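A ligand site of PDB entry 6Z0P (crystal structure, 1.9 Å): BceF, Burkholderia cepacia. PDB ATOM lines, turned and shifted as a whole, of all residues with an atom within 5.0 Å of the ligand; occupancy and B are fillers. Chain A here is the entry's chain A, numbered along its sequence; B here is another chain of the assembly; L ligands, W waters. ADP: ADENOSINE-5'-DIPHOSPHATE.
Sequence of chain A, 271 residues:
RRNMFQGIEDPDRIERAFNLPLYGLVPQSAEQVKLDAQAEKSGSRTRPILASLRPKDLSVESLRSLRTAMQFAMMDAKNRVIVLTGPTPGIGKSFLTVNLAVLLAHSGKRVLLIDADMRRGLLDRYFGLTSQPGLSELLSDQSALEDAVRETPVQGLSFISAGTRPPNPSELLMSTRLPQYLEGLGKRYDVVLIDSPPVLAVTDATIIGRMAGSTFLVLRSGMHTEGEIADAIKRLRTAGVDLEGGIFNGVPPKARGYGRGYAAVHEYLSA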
ATOM      1  N   VAL A  26     -13.963  -0.324  10.438  1.00  0.00           N
ATOM      2  CA  VAL A  26     -14.829  -1.425   9.912  1.00  0.00           C
ATOM      3  C   VAL A  26     -14.090  -2.738  10.104  1.00  0.00           C
ATOM      4  O   VAL A  26     -13.092  -2.980   9.439  1.00  0.00           O
ATOM      5  CB  VAL A  26     -15.204  -1.194   8.440  1.00  0.00           C
ATOM      6  CG1 VAL A  26     -16.043  -2.342   7.889  1.00  0.00           C
ATOM      7  CG2 VAL A  26     -15.930   0.130   8.258  1.00  0.00           C
ATOM      8  N   PRO A  27     -14.581  -3.621  10.991  1.00  0.00           N
ATOM      9  CA  PRO A  27     -13.941  -4.915  11.214  1.00  0.00           C
ATOM     10  C   PRO A  27     -13.924  -5.831   9.999  1.00  0.00           C
ATOM     11  O   PRO A  27     -14.788  -5.734   9.138  1.00  0.00           O
ATOM     12  CB  PRO A  27     -14.809  -5.606  12.272  1.00  0.00           C
ATOM     13  CG  PRO A  27     -15.655  -4.520  12.873  1.00  0.00           C
ATOM     14  CD  PRO A  27     -15.753  -3.414  11.839  1.00  0.00           C
ATOM     15  N   GLN A  28     -12.956  -6.733   9.974  1.00  0.00           N
ATOM     16  CA  GLN A  28     -12.990  -7.897   9.059  1.00  0.00           C
ATOM     17  C   GLN A  28     -14.194  -8.748   9.461  1.00  0.00           C
ATOM     18  O   GLN A  28     -14.155  -9.261  10.594  1.00  0.00           O
ATOM     19  CB  GLN A  28     -11.729  -8.752   9.189  1.00  0.00           C
ATOM     20  CG  GLN A  28     -10.697  -8.502   8.105  1.00  0.00           C
ATOM     21  CD  GLN A  28     -11.221  -8.880   6.740  1.00  0.00           C
ATOM     22  OE1 GLN A  28     -11.469  -8.033   5.895  1.00  0.00           O
ATOM     23  NE2 GLN A  28     -11.409 -10.179   6.528  1.00  0.00           N
ATOM     24  N   SER A  29     -15.210  -8.844   8.609  1.00  0.00           N
ATOM     25  CA  SER A  29     -16.435  -9.636   8.880  1.00  0.00           C
ATOM     26  C   SER A  29     -16.214 -11.077   8.426  1.00  0.00           C
ATOM     27  O   SER A  29     -15.938 -11.290   7.230  1.00  0.00           O
ATOM     28  CB  SER A  29     -17.649  -9.036   8.222  1.00  0.00           C
ATOM     29  OG  SER A  29     -18.585 -10.033   7.850  1.00  0.00           O
ATOM     30  N   GLN A  32     -18.819 -12.124   5.721  1.00  0.00           N
ATOM     31  CA  GLN A  32     -18.456 -11.631   4.380  1.00  0.00           C
ATOM     32  C   GLN A  32     -17.453 -12.628   3.772  1.00  0.00           C
ATOM     33  O   GLN A  32     -17.635 -13.012   2.609  1.00  0.00           O
ATOM     34  CB  GLN A  32     -17.891 -10.228   4.442  1.00  0.00           C
ATOM     35  CG  GLN A  32     -17.470  -9.695   3.082  1.00  0.00           C
ATOM     36  CD  GLN A  32     -18.645  -9.611   2.153  1.00  0.00           C
ATOM     37  OE1 GLN A  32     -19.666  -8.999   2.467  1.00  0.00           O
ATOM     38  NE2 GLN A  32     -18.525 -10.212   0.981  1.00  0.00           N
ATOM     39  N   VAL A  33     -16.448 -13.025   4.548  1.00  0.00           N
ATOM     40  CA  VAL A  33     -15.406 -13.984   4.062  1.00  0.00           C
ATOM     41  C   VAL A  33     -16.107 -15.255   3.577  1.00  0.00           C
ATOM     42  O   VAL A  33     -15.789 -15.717   2.469  1.00  0.00           O
ATOM     43  CB  VAL A  33     -14.352 -14.279   5.133  1.00  0.00           C
ATOM     44  CG1 VAL A  33     -13.444 -15.425   4.724  1.00  0.00           C
ATOM     45  CG2 VAL A  33     -13.533 -13.050   5.473  1.00  0.00           C
ATOM     46  N   ASP A  36     -18.106 -14.764   0.281  1.00  0.00           N
ATOM     47  CA  ASP A  36     -17.184 -14.607  -0.874  1.00  0.00           C
ATOM     48  C   ASP A  36     -16.677 -15.983  -1.301  1.00  0.00           C
ATOM     49  O   ASP A  36     -16.637 -16.244  -2.510  1.00  0.00           O
ATOM     50  CB  ASP A  36     -16.042 -13.643  -0.560  1.00  0.00           C
ATOM     51  CG  ASP A  36     -16.455 -12.180  -0.632  1.00  0.00           C
ATOM     52  OD1 ASP A  36     -17.216 -11.839  -1.548  1.00  0.00           O
ATOM     53  OD2 ASP A  36     -16.000 -11.409   0.223  1.00  0.00           O
ATOM     54  N   ARG A  47     -22.342 -10.495  -6.582  1.00  0.00           N
ATOM     55  CA  ARG A  47     -21.708 -10.299  -5.248  1.00  0.00           C
ATOM     56  C   ARG A  47     -22.804 -10.022  -4.222  1.00  0.00           C
ATOM     57  O   ARG A  47     -23.661  -9.165  -4.467  1.00  0.00           O
ATOM     58  CB  ARG A  47     -20.706  -9.142  -5.300  1.00  0.00           C
ATOM     59  CG  ARG A  47     -19.324  -9.550  -5.788  1.00  0.00           C
ATOM     60  CD  ARG A  47     -18.549  -8.397  -6.392  1.00  0.00           C
ATOM     61  NE  ARG A  47     -17.584  -7.817  -5.475  1.00  0.00           N
ATOM     62  CZ  ARG A  47     -16.403  -7.328  -5.820  1.00  0.00           C
ATOM     63  NH1 ARG A  47     -16.016  -7.348  -7.086  1.00  0.00           N
ATOM     64  NH2 ARG A  47     -15.606  -6.812  -4.909  1.00  0.00           N
ATOM     65  N   SER A  59     -19.702  -5.564  11.057  1.00  0.00           N
ATOM     66  CA  SER A  59     -19.189  -4.657  10.001  1.00  0.00           C
ATOM     67  C   SER A  59     -20.319  -3.736   9.540  1.00  0.00           C
ATOM     68  O   SER A  59     -20.094  -2.522   9.462  1.00  0.00           O
ATOM     69  CB  SER A  59     -18.582  -5.404   8.854  1.00  0.00           C
ATOM     70  OG  SER A  59     -17.485  -6.158   9.321  1.00  0.00           O
ATOM     71  N   THR A  88      -4.421   1.829  -3.253  1.00  0.00           N
ATOM     72  CA  THR A  88      -4.311   0.719  -4.235  1.00  0.00           C
ATOM     73  C   THR A  88      -5.603  -0.083  -4.272  1.00  0.00           C
ATOM     74  O   THR A  88      -6.446   0.064  -3.398  1.00  0.00           O
ATOM     75  CB  THR A  88      -3.230  -0.294  -3.847  1.00  0.00           C
ATOM     76  OG1 THR A  88      -3.650  -0.908  -2.635  1.00  0.00           O
ATOM     77  CG2 THR A  88      -1.836   0.285  -3.672  1.00  0.00           C
ATOM     78  N   PRO A  89      -5.769  -0.993  -5.260  1.00  0.00           N
ATOM     79  CA  PRO A  89      -6.803  -2.022  -5.183  1.00  0.00           C
ATOM     80  C   PRO A  89      -6.595  -3.010  -4.027  1.00  0.00           C
ATOM     81  O   PRO A  89      -5.496  -3.079  -3.497  1.00  0.00           O
ATOM     82  CB  PRO A  89      -6.645  -2.808  -6.502  1.00  0.00           C
ATOM     83  CG  PRO A  89      -5.947  -1.843  -7.431  1.00  0.00           C
ATOM     84  CD  PRO A  89      -5.059  -1.011  -6.540  1.00  0.00           C
ATOM     85  N   GLY A  90      -7.649  -3.740  -3.654  1.00  0.00           N
ATOM     86  CA  GLY A  90      -7.595  -4.812  -2.636  1.00  0.00           C
ATOM     87  C   GLY A  90      -7.800  -4.300  -1.224  1.00  0.00           C
ATOM     88  O   GLY A  90      -7.493  -5.057  -0.298  1.00  0.00           O
ATOM     89  N   ILE A  91      -8.329  -3.085  -1.065  1.00  0.00           N
ATOM     90  CA  ILE A  91      -8.460  -2.414   0.262  1.00  0.00           C
ATOM     91  C   ILE A  91      -9.885  -2.538   0.795  1.00  0.00           C
ATOM     92  O   ILE A  91     -10.093  -2.283   1.993  1.00  0.00           O
ATOM     93  CB  ILE A  91      -7.995  -0.946   0.153  1.00  0.00           C
ATOM     94  CG1 ILE A  91      -8.936  -0.110  -0.732  1.00  0.00           C
ATOM     95  CG2 ILE A  91      -6.546  -0.898  -0.312  1.00  0.00           C
ATOM     96  CD1 ILE A  91      -8.495   1.315  -0.937  1.00  0.00           C
ATOM     97  N   GLY A  92     -10.847  -2.922  -0.060  1.00  0.00           N
ATOM     98  CA  GLY A  92     -12.277  -3.031   0.308  1.00  0.00           C
ATOM     99  C   GLY A  92     -13.083  -1.815  -0.103  1.00  0.00           C
ATOM    100  O   GLY A  92     -14.144  -1.590   0.509  1.00  0.00           O
ATOM    101  N   LYS A  93     -12.651  -1.067  -1.120  1.00  0.00           N
ATOM    102  CA  LYS A  93     -13.375   0.180  -1.515  1.00  0.00           C
ATOM    103  C   LYS A  93     -14.718  -0.195  -2.158  1.00  0.00           C
ATOM    104  O   LYS A  93     -15.715   0.486  -1.869  1.00  0.00           O
ATOM    105  CB  LYS A  93     -12.510   1.089  -2.388  1.00  0.00           C
ATOM    106  CG  LYS A  93     -13.136   2.449  -2.659  1.00  0.00           C
ATOM    107  CD  LYS A  93     -12.182   3.566  -3.052  1.00  0.00           C
ATOM    108  CE  LYS A  93     -11.119   3.156  -4.052  1.00  0.00           C
ATOM    109  NZ  LYS A  93     -11.723   2.611  -5.297  1.00  0.00           N
ATOM    110  N   SER A  94     -14.768  -1.222  -3.020  1.00  0.00           N
ATOM    111  CA  SER A  94     -16.033  -1.750  -3.606  1.00  0.00           C
ATOM    112  C   SER A  94     -16.992  -2.101  -2.475  1.00  0.00           C
ATOM    113  O   SER A  94     -18.150  -1.656  -2.487  1.00  0.00           O
ATOM    114  CB  SER A  94     -15.791  -2.968  -4.435  1.00  0.00           C
ATOM    115  OG  SER A  94     -15.147  -2.656  -5.661  1.00  0.00           O
ATOM    116  N   PHE A  95     -16.506  -2.906  -1.536  1.00  0.00           N
ATOM    117  CA  PHE A  95     -17.300  -3.446  -0.402  1.00  0.00           C
ATOM    118  C   PHE A  95     -17.898  -2.302   0.420  1.00  0.00           C
ATOM    119  O   PHE A  95     -19.094  -2.355   0.719  1.00  0.00           O
ATOM    120  CB  PHE A  95     -16.440  -4.398   0.438  1.00  0.00           C
ATOM    121  CG  PHE A  95     -16.934  -4.635   1.838  1.00  0.00           C
ATOM    122  CD1 PHE A  95     -16.528  -3.818   2.884  1.00  0.00           C
ATOM    123  CD2 PHE A  95     -17.776  -5.694   2.123  1.00  0.00           C
ATOM    124  CE1 PHE A  95     -16.962  -4.044   4.175  1.00  0.00           C
ATOM    125  CE2 PHE A  95     -18.226  -5.910   3.426  1.00  0.00           C
ATOM    126  CZ  PHE A  95     -17.818  -5.093   4.448  1.00  0.00           C
ATOM    127  N   ARG A 120     -11.427  -1.518 -13.908  1.00  0.00           N
ATOM    128  CA  ARG A 120     -11.831  -2.806 -13.275  1.00  0.00           C
ATOM    129  C   ARG A 120     -13.346  -2.929 -13.283  1.00  0.00           C
ATOM    130  O   ARG A 120     -13.850  -4.004 -13.685  1.00  0.00           O
ATOM    131  CB  ARG A 120     -11.328  -2.880 -11.841  1.00  0.00           C
ATOM    132  CG  ARG A 120      -9.802  -2.826 -11.737  1.00  0.00           C
ATOM    133  CD  ARG A 120      -9.460  -2.171 -10.424  1.00  0.00           C
ATOM    134  NE  ARG A 120      -9.457  -3.210  -9.413  1.00  0.00           N
ATOM    135  CZ  ARG A 120      -9.881  -3.071  -8.164  1.00  0.00           C
ATOM    136  NH1 ARG A 120     -10.352  -1.907  -7.738  1.00  0.00           N
ATOM    137  NH2 ARG A 120      -9.833  -4.103  -7.353  1.00  0.00           N
ATOM    138  N   TYR A 126     -22.718  -6.493  -7.972  1.00  0.00           N
ATOM    139  CA  TYR A 126     -23.564  -6.447  -6.760  1.00  0.00           C
ATOM    140  C   TYR A 126     -25.038  -6.286  -7.133  1.00  0.00           C
ATOM    141  O   TYR A 126     -25.875  -6.332  -6.221  1.00  0.00           O
ATOM    142  CB  TYR A 126     -23.122  -5.316  -5.834  1.00  0.00           C
ATOM    143  CG  TYR A 126     -21.797  -5.521  -5.147  1.00  0.00           C
ATOM    144  CD1 TYR A 126     -21.704  -6.294  -4.007  1.00  0.00           C
ATOM    145  CD2 TYR A 126     -20.645  -4.934  -5.633  1.00  0.00           C
ATOM    146  CE1 TYR A 126     -20.493  -6.471  -3.356  1.00  0.00           C
ATOM    147  CE2 TYR A 126     -19.425  -5.105  -5.001  1.00  0.00           C
ATOM    148  CZ  TYR A 126     -19.349  -5.873  -3.862  1.00  0.00           C
ATOM    149  OH  TYR A 126     -18.149  -6.054  -3.233  1.00  0.00           O
ATOM    150  N   ARG A 220      -6.732  -0.225   4.264  1.00  0.00           N
ATOM    151  CA  ARG A 220      -6.977  -1.571   4.830  1.00  0.00           C
ATOM    152  C   ARG A 220      -5.907  -1.888   5.864  1.00  0.00           C
ATOM    153  O   ARG A 220      -4.728  -1.689   5.588  1.00  0.00           O
ATOM    154  CB  ARG A 220      -7.067  -2.636   3.750  1.00  0.00           C
ATOM    155  CG  ARG A 220      -7.394  -4.001   4.326  1.00  0.00           C
ATOM    156  CD  ARG A 220      -7.826  -4.985   3.275  1.00  0.00           C
ATOM    157  NE  ARG A 220      -8.795  -5.934   3.783  1.00  0.00           N
ATOM    158  CZ  ARG A 220      -9.470  -6.789   3.026  1.00  0.00           C
ATOM    159  NH1 ARG A 220      -9.267  -6.823   1.721  1.00  0.00           N
ATOM    160  NH2 ARG A 220     -10.333  -7.620   3.587  1.00  0.00           N
ATOM    161  N   ASN A 249     -10.390  -0.048   7.278  1.00  0.00           N
ATOM    162  CA  ASN A 249     -11.158  -1.276   6.969  1.00  0.00           C
ATOM    163  C   ASN A 249     -10.356  -2.524   7.340  1.00  0.00           C
ATOM    164  O   ASN A 249      -9.118  -2.446   7.405  1.00  0.00           O
ATOM    165  CB  ASN A 249     -11.591  -1.251   5.494  1.00  0.00           C
ATOM    166  CG  ASN A 249     -12.436  -2.439   5.088  1.00  0.00           C
ATOM    167  OD1 ASN A 249     -13.277  -2.901   5.855  1.00  0.00           O
ATOM    168  ND2 ASN A 249     -12.192  -2.950   3.895  1.00  0.00           N
ATOM    169  N   GLY A 250     -11.046  -3.631   7.615  1.00  0.00           N
ATOM    170  CA  GLY A 250     -10.432  -4.950   7.859  1.00  0.00           C
ATOM    171  C   GLY A 250      -9.809  -5.074   9.229  1.00  0.00           C
ATOM    172  O   GLY A 250      -8.927  -5.936   9.390  1.00  0.00           O
ATOM    173  N   ARG B 119      -5.618  -8.373 -12.625  1.00  0.00           N
ATOM    174  CA  ARG B 119      -6.701  -7.406 -12.308  1.00  0.00           C
ATOM    175  C   ARG B 119      -7.096  -6.658 -13.574  1.00  0.00           C
ATOM    176  O   ARG B 119      -8.262  -6.248 -13.655  1.00  0.00           O
ATOM    177  CB  ARG B 119      -6.281  -6.374 -11.272  1.00  0.00           C
ATOM    178  CG  ARG B 119      -6.197  -6.913  -9.859  1.00  0.00           C
ATOM    179  CD  ARG B 119      -5.928  -5.791  -8.896  1.00  0.00           C
ATOM    180  NE  ARG B 119      -5.524  -6.276  -7.585  1.00  0.00           N
ATOM    181  CZ  ARG B 119      -6.367  -6.580  -6.611  1.00  0.00           C
ATOM    182  NH1 ARG B 119      -7.669  -6.467  -6.791  1.00  0.00           N
ATOM    183  NH2 ARG B 119      -5.906  -7.007  -5.454  1.00  0.00           N
HETATM  184  PB  ADP L   1     -11.172  -2.976  -3.923  1.00  0.00           P
HETATM  185  O1B ADP L   1     -10.580  -2.032  -2.902  1.00  0.00           O
HETATM  186  O2B ADP L   1     -10.191  -3.384  -4.995  1.00  0.00           O
HETATM  187  O3B ADP L   1     -12.473  -2.458  -4.502  1.00  0.00           O
HETATM  188  PA  ADP L   1     -12.932  -4.984  -2.675  1.00  0.00           P
HETATM  189  O1A ADP L   1     -13.839  -3.920  -2.164  1.00  0.00           O
HETATM  190  O2A ADP L   1     -13.405  -5.844  -3.801  1.00  0.00           O
HETATM  191  O3A ADP L   1     -11.541  -4.316  -3.108  1.00  0.00           O
HETATM  192  O5' ADP L   1     -12.453  -5.907  -1.451  1.00  0.00           O
HETATM  193  C5' ADP L   1     -11.569  -7.023  -1.725  1.00  0.00           C
HETATM  194  C4' ADP L   1     -12.176  -8.289  -1.163  1.00  0.00           C
HETATM  195  O4' ADP L   1     -12.173  -8.203   0.287  1.00  0.00           O
HETATM  196  C3' ADP L   1     -13.633  -8.559  -1.556  1.00  0.00           C
HETATM  197  O3' ADP L   1     -13.886  -9.959  -1.695  1.00  0.00           O
HETATM  198  C2' ADP L   1     -14.409  -7.966  -0.380  1.00  0.00           C
HETATM  199  O2' ADP L   1     -15.689  -8.548  -0.217  1.00  0.00           O
HETATM  200  C1' ADP L   1     -13.483  -8.306   0.785  1.00  0.00           C
HETATM  201  N9  ADP L   1     -13.617  -7.415   1.927  1.00  0.00           N
HETATM  202  C8  ADP L   1     -13.429  -6.054   1.921  1.00  0.00           C
HETATM  203  N7  ADP L   1     -13.618  -5.495   3.090  1.00  0.00           N
HETATM  204  C5  ADP L   1     -13.933  -6.565   3.924  1.00  0.00           C
HETATM  205  C6  ADP L   1     -14.242  -6.623   5.305  1.00  0.00           C
HETATM  206  N6  ADP L   1     -14.272  -5.558   6.096  1.00  0.00           N
HETATM  207  N1  ADP L   1     -14.510  -7.836   5.823  1.00  0.00           N
HETATM  208  C2  ADP L   1     -14.474  -8.908   5.012  1.00  0.00           C
HETATM  209  N3  ADP L   1     -14.200  -8.966   3.718  1.00  0.00           N
HETATM  210  C4  ADP L   1     -13.938  -7.746   3.221  1.00  0.00           C
HETATM  211  O   HOH W   1     -13.101   0.122  -5.604  1.00  0.00           O
HETATM  212  O   HOH W   2     -10.034  -6.432  -5.271  1.00  0.00           O
HETATM  213  O   HOH W   3      -9.207   0.093  -4.178  1.00  0.00           O
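The side-chain hydroxyl (OG) of Ser 29 sits at hydrogen-bond distance from the backbone NH (N) of Gln 32, at 3.0 Å. O of Gly 90 is in hydrogen-bond range of NH1 of Arg 220 (3.2 Å). O of Ile 91 is in hydrogen-bond range of ND2 of Asn 249 (2.9 Å). OG of Ser 59 sits at hydrogen-bond distance from O of Pro 27 (2.7 Å). The side-chain hydroxyl of Tyr 126 lies within hydrogen-bond range of the guanidinium group of Arg 47 (2.9 Å). OE1 of Gln 28 lies within hydrogen-bond range of NH2 of Arg 220 (2.6 Å). NE2 of Gln 32 lies within hydrogen-bond range of OD2 of Asp 36 (2.9 Å).
An oxygen (O2') of the ligand sits close to the side-chain amide nitrogen of Gln 32, 3.5 Å away. Pro 89 touches the ligand (CA to O2B, 3.7 Å). Arg 220 touches the ligand (NH1 to O4', 3.5 Å). Hydrophobic or aromatic side chains that line the ligand: Pro 89, Ile 91 and Phe 95. Of the 23 residues printed, 16 come within 4 Å of the ligand.
Water W3 lies within hydrogen-bond range of O1B of the ligand (2.8 Å) and O of Thr 88 (2.9 Å). Water W1 lies within hydrogen-bond range of NZ of Lys 93 (2.9 Å), O3B of the ligand (2.9 Å) and N of Ser 94 (3.4 Å). Water W2 lies within hydrogen-bond range of NH1 of Arg 119 of chain B, O2B of the ligand and NH2 of Arg 120.
An oxygen (O2') of the ligand is in hydrogen-bond range of the side-chain carboxylate of Asp 36, at 2.9 Å. O1B of the ligand sits at hydrogen-bond distance from N of Lys 93, at 2.9 Å. The backbone NH (N) of Gly 92 lies within hydrogen-bond range of an oxygen (O1B) of the ligand. The backbone NH (N) of Ser 94 is in hydrogen-bond range of an oxygen (O1A) of the ligand. OG of Ser 94 is in hydrogen-bond range of O3B of the ligand. O of Pro 27 lies within hydrogen-bond range of N6 of the ligand, 3.1 Å away. The guanidinium group (NH2) of Arg 47 is in salt-bridge range of an oxygen (O2A) of the ligand, at 2.6 Å. N of Ile 91 sits at hydrogen-bond distance from O1B of the ligand, at 3.1 Å. N1 of the ligand is in hydrogen-bond range of N of Ser 29 (3.0 Å). A nitrogen (N6) of the ligand is in hydrogen-bond range of the side-chain amide oxygen of Asn 249, at 2.8 Å. The side-chain amide oxygen (OE1) of Gln 28 lies close to a nitrogen (N1) of the ligand, at 3.0 Å. O1A of the ligand is in hydrogen-bond range of N of Phe 95, 2.9 Å away. O2B of the ligand lies within hydrogen-bond range of N of Gly 90 (2.9 Å). An oxygen (O2B) of the ligand lies within salt-bridge range of the guanidinium group (NH2) of Arg 120, at 2.5 Å.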
